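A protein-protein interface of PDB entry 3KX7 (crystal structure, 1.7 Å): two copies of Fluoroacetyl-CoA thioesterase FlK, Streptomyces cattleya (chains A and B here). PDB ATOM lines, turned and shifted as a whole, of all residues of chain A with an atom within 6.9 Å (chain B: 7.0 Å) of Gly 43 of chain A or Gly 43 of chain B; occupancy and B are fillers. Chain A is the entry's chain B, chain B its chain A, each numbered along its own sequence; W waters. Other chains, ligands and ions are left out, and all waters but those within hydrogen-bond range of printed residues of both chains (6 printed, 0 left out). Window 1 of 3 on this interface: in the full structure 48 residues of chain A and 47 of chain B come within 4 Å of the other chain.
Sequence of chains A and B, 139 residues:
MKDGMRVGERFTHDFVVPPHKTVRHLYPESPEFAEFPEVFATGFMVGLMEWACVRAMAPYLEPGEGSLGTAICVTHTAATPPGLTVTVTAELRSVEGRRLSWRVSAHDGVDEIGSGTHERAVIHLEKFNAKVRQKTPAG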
ATOM      1  N   VAL A  23      23.674  30.900   8.448  1.00  0.00           N
ATOM      2  CA  VAL A  23      23.431  30.386   9.792  1.00  0.00           C
ATOM      3  C   VAL A  23      22.688  31.390  10.667  1.00  0.00           C
ATOM      4  O   VAL A  23      21.888  30.996  11.510  1.00  0.00           O
ATOM      5  CB  VAL A  23      24.684  29.777  10.500  1.00  0.00           C
ATOM      6  CG1 VAL A  23      25.629  30.864  11.007  1.00  0.00           C
ATOM      7  CG2 VAL A  23      24.250  28.880  11.635  1.00  0.00           C
ATOM      8  N   LEU A  26      19.288  30.710  10.011  1.00  0.00           N
ATOM      9  CA  LEU A  26      18.868  29.442  10.596  1.00  0.00           C
ATOM     10  C   LEU A  26      18.395  29.628  12.032  1.00  0.00           C
ATOM     11  O   LEU A  26      17.354  29.114  12.402  1.00  0.00           O
ATOM     12  CB  LEU A  26      19.999  28.422  10.519  1.00  0.00           C
ATOM     13  CG  LEU A  26      19.678  26.956  10.841  1.00  0.00           C
ATOM     14  CD1 LEU A  26      18.699  26.348   9.841  1.00  0.00           C
ATOM     15  CD2 LEU A  26      20.985  26.206  10.863  1.00  0.00           C
ATOM     16  N   TYR A  27      19.151  30.383  12.826  1.00  0.00           N
ATOM     17  CA  TYR A  27      18.732  30.733  14.168  1.00  0.00           C
ATOM     18  C   TYR A  27      18.820  32.255  14.395  1.00  0.00           C
ATOM     19  O   TYR A  27      19.850  32.763  14.861  1.00  0.00           O
ATOM     20  CB  TYR A  27      19.514  29.941  15.223  1.00  0.00           C
ATOM     21  CG  TYR A  27      18.948  28.557  15.478  1.00  0.00           C
ATOM     22  CD1 TYR A  27      17.985  28.354  16.471  1.00  0.00           C
ATOM     23  CD2 TYR A  27      19.348  27.452  14.701  1.00  0.00           C
ATOM     24  CE1 TYR A  27      17.453  27.099  16.711  1.00  0.00           C
ATOM     25  CE2 TYR A  27      18.817  26.184  14.942  1.00  0.00           C
ATOM     26  CZ  TYR A  27      17.881  26.012  15.934  1.00  0.00           C
ATOM     27  OH  TYR A  27      17.317  24.774  16.175  1.00  0.00           O
ATOM     28  N   PHE A  40      26.174  29.630   3.109  1.00  0.00           N
ATOM     29  CA  PHE A  40      25.109  28.627   3.198  1.00  0.00           C
ATOM     30  C   PHE A  40      25.313  27.757   4.448  1.00  0.00           C
ATOM     31  O   PHE A  40      26.368  27.143   4.626  1.00  0.00           O
ATOM     32  CB  PHE A  40      25.130  27.801   1.901  1.00  0.00           C
ATOM     33  CG  PHE A  40      23.959  26.869   1.723  1.00  0.00           C
ATOM     34  CD1 PHE A  40      24.185  25.575   1.245  1.00  0.00           C
ATOM     35  CD2 PHE A  40      22.646  27.287   1.955  1.00  0.00           C
ATOM     36  CE1 PHE A  40      23.110  24.686   1.038  1.00  0.00           C
ATOM     37  CE2 PHE A  40      21.558  26.412   1.734  1.00  0.00           C
ATOM     38  CZ  PHE A  40      21.797  25.115   1.280  1.00  0.00           C
ATOM     39  N   ALA A  41      24.310  27.707   5.323  1.00  0.00           N
ATOM     40  CA  ALA A  41      24.486  27.012   6.601  1.00  0.00           C
ATOM     41  C   ALA A  41      24.405  25.510   6.422  1.00  0.00           C
ATOM     42  O   ALA A  41      23.676  25.029   5.566  1.00  0.00           O
ATOM     43  CB  ALA A  41      23.496  27.483   7.623  1.00  0.00           C
ATOM     44  N   THR A  42      25.152  24.783   7.252  1.00  0.00           N
ATOM     45  CA  THR A  42      25.133  23.332   7.244  1.00  0.00           C
ATOM     46  C   THR A  42      23.705  22.815   7.450  1.00  0.00           C
ATOM     47  O   THR A  42      23.269  21.911   6.733  1.00  0.00           O
ATOM     48  CB  THR A  42      26.058  22.732   8.321  1.00  0.00           C
ATOM     49  OG1 THR A  42      27.381  23.270   8.169  1.00  0.00           O
ATOM     50  CG2 THR A  42      26.099  21.213   8.189  1.00  0.00           C
ATOM     51  N   GLY A  43      22.974  23.404   8.392  1.00  0.00           N
ATOM     52  CA  GLY A  43      21.592  22.949   8.644  1.00  0.00           C
ATOM     53  C   GLY A  43      20.713  23.107   7.423  1.00  0.00           C
ATOM     54  O   GLY A  43      19.802  22.291   7.185  1.00  0.00           O
ATOM     55  N   PHE A  44      20.928  24.189   6.669  1.00  0.00           N
ATOM     56  CA  PHE A  44      20.194  24.373   5.418  1.00  0.00           C
ATOM     57  C   PHE A  44      20.647  23.365   4.358  1.00  0.00           C
ATOM     58  O   PHE A  44      19.810  22.829   3.640  1.00  0.00           O
ATOM     59  CB  PHE A  44      20.240  25.825   4.912  1.00  0.00           C
ATOM     60  CG  PHE A  44      19.363  26.782   5.701  1.00  0.00           C
ATOM     61  CD1 PHE A  44      17.978  26.566   5.807  1.00  0.00           C
ATOM     62  CD2 PHE A  44      19.901  27.916   6.299  1.00  0.00           C
ATOM     63  CE1 PHE A  44      17.165  27.443   6.511  1.00  0.00           C
ATOM     64  CE2 PHE A  44      19.072  28.817   7.012  1.00  0.00           C
ATOM     65  CZ  PHE A  44      17.708  28.576   7.106  1.00  0.00           C
ATOM     66  N   MET A  45      21.954  23.065   4.293  1.00  0.00           N
ATOM     67  CA  MET A  45      22.426  22.051   3.343  1.00  0.00           C
ATOM     68  C   MET A  45      21.799  20.690   3.659  1.00  0.00           C
ATOM     69  O   MET A  45      21.344  19.981   2.749  1.00  0.00           O
ATOM     70  CB  MET A  45      23.954  21.973   3.325  1.00  0.00           C
ATOM     71  CG  MET A  45      24.439  20.923   2.328  1.00  0.00           C
ATOM     72  SD  MET A  45      26.232  20.740   2.292  1.00  0.00           S
ATOM     73  CE  MET A  45      26.485  19.848   3.822  1.00  0.00           C
ATOM     74  N   VAL A  46      21.744  20.351   4.942  1.00  0.00           N
ATOM     75  CA  VAL A  46      21.085  19.103   5.396  1.00  0.00           C
ATOM     76  C   VAL A  46      19.632  19.098   4.901  1.00  0.00           C
ATOM     77  O   VAL A  46      19.162  18.107   4.299  1.00  0.00           O
ATOM     78  CB  VAL A  46      21.176  18.961   6.930  1.00  0.00           C
ATOM     79  CG1 VAL A  46      20.209  17.875   7.435  1.00  0.00           C
ATOM     80  CG2 VAL A  46      22.602  18.572   7.322  1.00  0.00           C
ATOM     81  N   GLY A  47      18.913  20.212   5.115  1.00  0.00           N
ATOM     82  CA  GLY A  47      17.507  20.275   4.667  1.00  0.00           C
ATOM     83  C   GLY A  47      17.375  20.153   3.150  1.00  0.00           C
ATOM     84  O   GLY A  47      16.422  19.578   2.655  1.00  0.00           O
ATOM     85  N   LEU A  48      18.350  20.702   2.416  1.00  0.00           N
ATOM     86  CA  LEU A  48      18.339  20.650   0.955  1.00  0.00           C
ATOM     87  C   LEU A  48      18.558  19.198   0.506  1.00  0.00           C
ATOM     88  O   LEU A  48      17.916  18.721  -0.423  1.00  0.00           O
ATOM     89  CB  LEU A  48      19.450  21.538   0.372  1.00  0.00           C
ATOM     90  CG  LEU A  48      19.360  21.778  -1.139  1.00  0.00           C
ATOM     91  CD1 LEU A  48      18.040  22.459  -1.518  1.00  0.00           C
ATOM     92  CD2 LEU A  48      20.595  22.633  -1.592  1.00  0.00           C
ATOM     93  N   GLU A  50      17.723  16.471   2.253  1.00  0.00           N
ATOM     94  CA  GLU A  50      16.441  15.798   2.530  1.00  0.00           C
ATOM     95  C   GLU A  50      15.445  16.098   1.436  1.00  0.00           C
ATOM     96  O   GLU A  50      14.733  15.209   0.980  1.00  0.00           O
ATOM     97  CB  GLU A  50      15.839  16.252   3.866  1.00  0.00           C
ATOM     98  CG  GLU A  50      16.646  15.842   5.097  1.00  0.00           C
ATOM     99  CD  GLU A  50      15.791  15.821   6.368  1.00  0.00           C
ATOM    100  OE1 GLU A  50      14.672  15.261   6.354  1.00  0.00           O
ATOM    101  OE2 GLU A  50      16.243  16.373   7.389  1.00  0.00           O
ATOM    102  N   HIS A  76      31.037  19.033   5.173  1.00  0.00           N
ATOM    103  CA  HIS A  76      30.689  20.331   4.620  1.00  0.00           C
ATOM    104  C   HIS A  76      32.006  21.072   4.457  1.00  0.00           C
ATOM    105  O   HIS A  76      32.473  21.742   5.390  1.00  0.00           O
ATOM    106  CB  HIS A  76      29.743  21.099   5.545  1.00  0.00           C
ATOM    107  CG  HIS A  76      29.064  22.266   4.889  1.00  0.00           C
ATOM    108  ND1 HIS A  76      28.274  23.148   5.588  1.00  0.00           N
ATOM    109  CD2 HIS A  76      29.057  22.698   3.603  1.00  0.00           C
ATOM    110  CE1 HIS A  76      27.800  24.066   4.765  1.00  0.00           C
ATOM    111  NE2 HIS A  76      28.257  23.813   3.553  1.00  0.00           N
ATOM    112  N   LEU B  26      11.883  25.305   7.689  1.00  0.00           N
ATOM    113  CA  LEU B  26      13.282  25.230   7.222  1.00  0.00           C
ATOM    114  C   LEU B  26      13.351  25.645   5.768  1.00  0.00           C
ATOM    115  O   LEU B  26      14.211  26.443   5.396  1.00  0.00           O
ATOM    116  CB  LEU B  26      13.855  23.813   7.392  1.00  0.00           C
ATOM    117  CG  LEU B  26      15.370  23.739   7.192  1.00  0.00           C
ATOM    118  CD1 LEU B  26      16.114  24.430   8.330  1.00  0.00           C
ATOM    119  CD2 LEU B  26      15.785  22.279   7.097  1.00  0.00           C
ATOM    120  N   TYR B  27      12.420  25.135   4.950  1.00  0.00           N
ATOM    121  CA  TYR B  27      12.304  25.515   3.553  1.00  0.00           C
ATOM    122  C   TYR B  27      10.873  25.901   3.209  1.00  0.00           C
ATOM    123  O   TYR B  27      10.119  25.080   2.700  1.00  0.00           O
ATOM    124  CB  TYR B  27      12.792  24.384   2.614  1.00  0.00           C
ATOM    125  CG  TYR B  27      14.291  24.414   2.474  1.00  0.00           C
ATOM    126  CD1 TYR B  27      14.901  25.253   1.541  1.00  0.00           C
ATOM    127  CD2 TYR B  27      15.099  23.654   3.313  1.00  0.00           C
ATOM    128  CE1 TYR B  27      16.298  25.310   1.420  1.00  0.00           C
ATOM    129  CE2 TYR B  27      16.488  23.696   3.197  1.00  0.00           C
ATOM    130  CZ  TYR B  27      17.078  24.536   2.251  1.00  0.00           C
ATOM    131  OH  TYR B  27      18.459  24.608   2.145  1.00  0.00           O
ATOM    132  N   PHE B  40      10.117  19.194  14.982  1.00  0.00           N
ATOM    133  CA  PHE B  40      11.451  19.813  14.903  1.00  0.00           C
ATOM    134  C   PHE B  40      12.277  19.251  13.725  1.00  0.00           C
ATOM    135  O   PHE B  40      12.528  18.040  13.657  1.00  0.00           O
ATOM    136  CB  PHE B  40      12.148  19.530  16.245  1.00  0.00           C
ATOM    137  CG  PHE B  40      13.402  20.360  16.510  1.00  0.00           C
ATOM    138  CD1 PHE B  40      13.472  21.724  16.201  1.00  0.00           C
ATOM    139  CD2 PHE B  40      14.473  19.768  17.171  1.00  0.00           C
ATOM    140  CE1 PHE B  40      14.644  22.493  16.513  1.00  0.00           C
ATOM    141  CE2 PHE B  40      15.644  20.507  17.488  1.00  0.00           C
ATOM    142  CZ  PHE B  40      15.730  21.882  17.159  1.00  0.00           C
ATOM    143  N   ALA B  41      12.685  20.115  12.791  1.00  0.00           N
ATOM    144  CA  ALA B  41      13.429  19.649  11.599  1.00  0.00           C
ATOM    145  C   ALA B  41      14.839  19.179  11.933  1.00  0.00           C
ATOM    146  O   ALA B  41      15.496  19.735  12.786  1.00  0.00           O
ATOM    147  CB  ALA B  41      13.535  20.779  10.556  1.00  0.00           C
ATOM    148  N   THR B  42      15.339  18.193  11.192  1.00  0.00           N
ATOM    149  CA  THR B  42      16.722  17.767  11.390  1.00  0.00           C
ATOM    150  C   THR B  42      17.705  18.911  11.168  1.00  0.00           C
ATOM    151  O   THR B  42      18.625  19.099  11.960  1.00  0.00           O
ATOM    152  CB  THR B  42      17.096  16.543  10.487  1.00  0.00           C
ATOM    153  OG1 THR B  42      16.152  15.475  10.702  1.00  0.00           O
ATOM    154  CG2 THR B  42      18.520  16.089  10.812  1.00  0.00           C
ATOM    155  N   GLY B  43      17.485  19.705  10.122  1.00  0.00           N
ATOM    156  CA  GLY B  43      18.393  20.821   9.840  1.00  0.00           C
ATOM    157  C   GLY B  43      18.432  21.820  11.002  1.00  0.00           C
ATOM    158  O   GLY B  43      19.481  22.406  11.292  1.00  0.00           O
ATOM    159  N   PHE B  44      17.289  22.041  11.640  1.00  0.00           N
ATOM    160  CA  PHE B  44      17.254  22.867  12.861  1.00  0.00           C
ATOM    161  C   PHE B  44      17.928  22.175  14.058  1.00  0.00           C
ATOM    162  O   PHE B  44      18.558  22.854  14.886  1.00  0.00           O
ATOM    163  CB  PHE B  44      15.817  23.298  13.231  1.00  0.00           C
ATOM    164  CG  PHE B  44      15.243  24.382  12.344  1.00  0.00           C
ATOM    165  CD1 PHE B  44      15.936  25.572  12.097  1.00  0.00           C
ATOM    166  CD2 PHE B  44      13.996  24.224  11.763  1.00  0.00           C
ATOM    167  CE1 PHE B  44      15.380  26.579  11.292  1.00  0.00           C
ATOM    168  CE2 PHE B  44      13.459  25.203  10.928  1.00  0.00           C
ATOM    169  CZ  PHE B  44      14.137  26.381  10.701  1.00  0.00           C
ATOM    170  N   MET B  45      17.762  20.850  14.189  1.00  0.00           N
ATOM    171  CA  MET B  45      18.465  20.134  15.254  1.00  0.00           C
ATOM    172  C   MET B  45      19.960  20.304  15.067  1.00  0.00           C
ATOM    173  O   MET B  45      20.685  20.642  16.022  1.00  0.00           O
ATOM    174  CB  MET B  45      18.104  18.642  15.308  1.00  0.00           C
ATOM    175  CG  MET B  45      18.768  17.963  16.511  1.00  0.00           C
ATOM    176  SD  MET B  45      18.285  16.208  16.679  1.00  0.00           S
ATOM    177  CE  MET B  45      19.153  15.519  15.242  1.00  0.00           C
ATOM    178  N   VAL B  46      20.429  20.088  13.839  1.00  0.00           N
ATOM    179  CA  VAL B  46      21.843  20.286  13.511  1.00  0.00           C
ATOM    180  C   VAL B  46      22.314  21.694  13.886  1.00  0.00           C
ATOM    181  O   VAL B  46      23.350  21.846  14.547  1.00  0.00           O
ATOM    182  CB  VAL B  46      22.129  19.958  12.033  1.00  0.00           C
ATOM    183  CG1 VAL B  46      23.528  20.438  11.623  1.00  0.00           C
ATOM    184  CG2 VAL B  46      21.989  18.475  11.809  1.00  0.00           C
ATOM    185  N   GLY B  47      21.526  22.702  13.507  1.00  0.00           N
ATOM    186  CA  GLY B  47      21.837  24.102  13.841  1.00  0.00           C
ATOM    187  C   GLY B  47      21.906  24.353  15.356  1.00  0.00           C
ATOM    188  O   GLY B  47      22.785  25.086  15.831  1.00  0.00           O
ATOM    189  N   LEU B  48      20.996  23.731  16.109  1.00  0.00           N
ATOM    190  CA  LEU B  48      21.010  23.813  17.587  1.00  0.00           C
ATOM    191  C   LEU B  48      22.284  23.180  18.175  1.00  0.00           C
ATOM    192  O   LEU B  48      22.913  23.722  19.098  1.00  0.00           O
ATOM    193  CB  LEU B  48      19.774  23.151  18.177  1.00  0.00           C
ATOM    194  CG  LEU B  48      19.581  23.299  19.694  1.00  0.00           C
ATOM    195  CD1 LEU B  48      19.377  24.784  20.075  1.00  0.00           C
ATOM    196  CD2 LEU B  48      18.404  22.453  20.144  1.00  0.00           C
ATOM    197  N   GLU B  50      25.191  22.851  16.525  1.00  0.00           N
ATOM    198  CA  GLU B  50      26.254  23.800  16.181  1.00  0.00           C
ATOM    199  C   GLU B  50      26.300  24.941  17.193  1.00  0.00           C
ATOM    200  O   GLU B  50      27.346  25.247  17.736  1.00  0.00           O
ATOM    201  CB  GLU B  50      26.064  24.387  14.782  1.00  0.00           C
ATOM    202  CG  GLU B  50      26.490  23.445  13.683  1.00  0.00           C
ATOM    203  CD  GLU B  50      26.734  24.143  12.350  1.00  0.00           C
ATOM    204  OE1 GLU B  50      27.436  25.195  12.286  1.00  0.00           O
ATOM    205  OE2 GLU B  50      26.226  23.608  11.347  1.00  0.00           O
ATOM    206  N   ILE B  72      28.912  16.884  10.016  1.00  0.00           N
ATOM    207  CA  ILE B  72      27.878  16.558  10.977  1.00  0.00           C
ATOM    208  C   ILE B  72      27.476  15.116  10.692  1.00  0.00           C
ATOM    209  O   ILE B  72      27.224  14.766   9.545  1.00  0.00           O
ATOM    210  CB  ILE B  72      26.650  17.531  10.897  1.00  0.00           C
ATOM    211  CG1 ILE B  72      25.623  17.228  12.019  1.00  0.00           C
ATOM    212  CG2 ILE B  72      25.988  17.474   9.494  1.00  0.00           C
ATOM    213  CD1 ILE B  72      26.105  17.584  13.427  1.00  0.00           C
ATOM    214  N   HIS B  76      18.543  10.908  14.102  1.00  0.00           N
ATOM    215  CA  HIS B  76      17.398  11.673  14.574  1.00  0.00           C
ATOM    216  C   HIS B  76      16.310  10.623  14.770  1.00  0.00           C
ATOM    217  O   HIS B  76      15.686  10.213  13.796  1.00  0.00           O
ATOM    218  CB  HIS B  76      16.984  12.709  13.520  1.00  0.00           C
ATOM    219  CG  HIS B  76      16.117  13.800  14.075  1.00  0.00           C
ATOM    220  ND1 HIS B  76      15.762  14.915  13.352  1.00  0.00           N
ATOM    221  CD2 HIS B  76      15.572  13.961  15.308  1.00  0.00           C
ATOM    222  CE1 HIS B  76      15.009  15.706  14.102  1.00  0.00           C
ATOM    223  NE2 HIS B  76      14.871  15.146  15.292  1.00  0.00           N
HETATM  224  O   HOH W   1      17.448  13.916   8.465  1.00  0.00           O
HETATM  225  O   HOH W   2      23.823  24.372  10.797  1.00  0.00           O
HETATM  226  O   HOH W   3      26.448  26.422   9.400  1.00  0.00           O
HETATM  227  O   HOH W   4      16.190  18.950   7.816  1.00  0.00           O
HETATM  228  O   HOH W   5      13.652  17.244   9.089  1.00  0.00           O
HETATM  229  O   HOH W   6      13.797  14.666   9.629  1.00  0.00           O
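Water W2 lies within hydrogen-bond range of OE2 of Glu 50 of chain B (2.6 Å) and N of Gly 43 of chain A (2.7 Å).
Water W4 lies within hydrogen-bond range of OE2 of Glu 50 of chain A and N of Gly 43 of chain B.
Water W6 lies within hydrogen-bond range of OG1 of Thr 42 of chain B (2.7 Å) and OE1 of Glu 50 of chain A (3.4 Å).
Water W5 lies within hydrogen-bond range of the backbone NH (N) of Thr 42 of chain B (2.9 Å) and the side-chain carboxylate (OE2) of Glu 50 of chain A (3.2 Å).
Water W1 bridges the side-chain carboxylate of Glu 50 of chain A (2.9 Å) and the side-chain hydroxyl of Thr 42 of chain B (3.0 Å).
Water W3 lies within hydrogen-bond range of N of Thr 42 of chain A (3.0 Å) and OE1 of Glu 50 of chain B (3.3 Å).
Among the printed residues, merely in contact across the chains: Phe 44 of chain A with Leu 26 of chain B, Gly 43 of chain A with Gly 43 of chain B, Leu 26 of chain A with Phe 44 of chain B, Tyr 27 of chain A with Phe 40 of chain B, Tyr 27 of chain A with Leu 48 of chain B, Phe 40 of chain A with Tyr 27 of chain B, Leu 26 of chain A with Leu 26 of chain B, Gly 47 of chain A with Leu 26 of chain B, Leu 48 of chain A with Tyr 27 of chain B, Tyr 27 of chain A with Gly 47 of chain B, Gly 47 of chain A with Tyr 27 of chain B, Leu 26 of chain A with Gly 47 of chain B and Thr 42 of chain A with Ile 72 of chain B.
Printed residues of chain A that touch a printed residue of chain B: Leu 26, Tyr 27, Phe 40, Thr 42, Gly 43, Phe 44, Gly 47, Leu 48 and Glu 50.
Hydrophobic or aromatic side chains of chain A within 4 Å of the printed part of chain B: Leu 26, Tyr 27, Phe 40, Phe 44 and Leu 48.
Of the 14 printed residues of chain B, 10 touch a printed residue of chain A.
Among the printed residues, 17 pairs touch across the chains.
The side-chain hydroxyl (OG1) of Thr 42 of chain B is in hydrogen-bond range of a ring nitrogen (ND1) of His 76 of chain B, at 2.7 Å.
The side-chain hydroxyl (OG1) of Thr 42 of chain A is in hydrogen-bond range of a ring nitrogen (ND1) of His 76 of chain A (2.7 Å).
Leu 26 of chain A touches Gly 47 of chain B, and with the chains exchanged Gly 47 of chain A touches Leu 26 of chain B.
Tyr 27 of chain A touches Leu 48 of chain B, and with the chains exchanged Leu 48 of chain A touches Tyr 27 of chain B.
Thr 42 of chain A touches Glu 50 of chain B, and with the chains exchanged Glu 50 of chain A touches Thr 42 of chain B.
Gly 43 of chain A touches its own counterpart, Gly 43 of chain B.
Positions printed for both chains: 26, 27, 40, 41, 42, 43, 44, 45, 46, 47, 48, 50 and 76.
Of the 17 pairs that touch across the chains among the printed residues, 16 have their exchanged pair printed and touching as well.
OH of Tyr 27 of chain B lies within hydrogen-bond range of O of Phe 44 of chain A, 2.7 Å away.
OG1 of Thr 42 of chain B sits close to OE2 of Glu 50 of chain A (3.4 Å).
The backbone carbonyl oxygen of Phe 44 of chain B is in hydrogen-bond range of the side-chain hydroxyl of Tyr 27 of chain A, at 2.6 Å.
The side-chain carboxylate of Glu 50 of chain B sits close to the side-chain hydroxyl of Thr 42 of chain A, 3.4 Å away.
Printed residues of chain B within 4 Å of Gly 43 of chain A: Gly 43.
Gly 43 of chain B touches just one residue of chain A: Gly 43.
Of the printed residues of chain A, Leu 26 of chain B touches Leu 26, Phe 44 and Gly 47.
Of the printed residues of chain B, Phe 40 of chain A touches Tyr 27.
Printed residues of chain B within 4 Å of Phe 44 of chain A: Leu 26 (3.3 Å) and Tyr 27 (2.7 Å).
Of the printed residues of chain A, Phe 44 of chain B touches Leu 26 (3.4 Å) and Tyr 27 (2.6 Å).
Printed residues of chain A within 4 Å of Thr 42 of chain B: Glu 50.
The nearest printed residue of chain A that does not touch Glu 50 of chain B is Gly 43 of chain A (4.4 Å).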
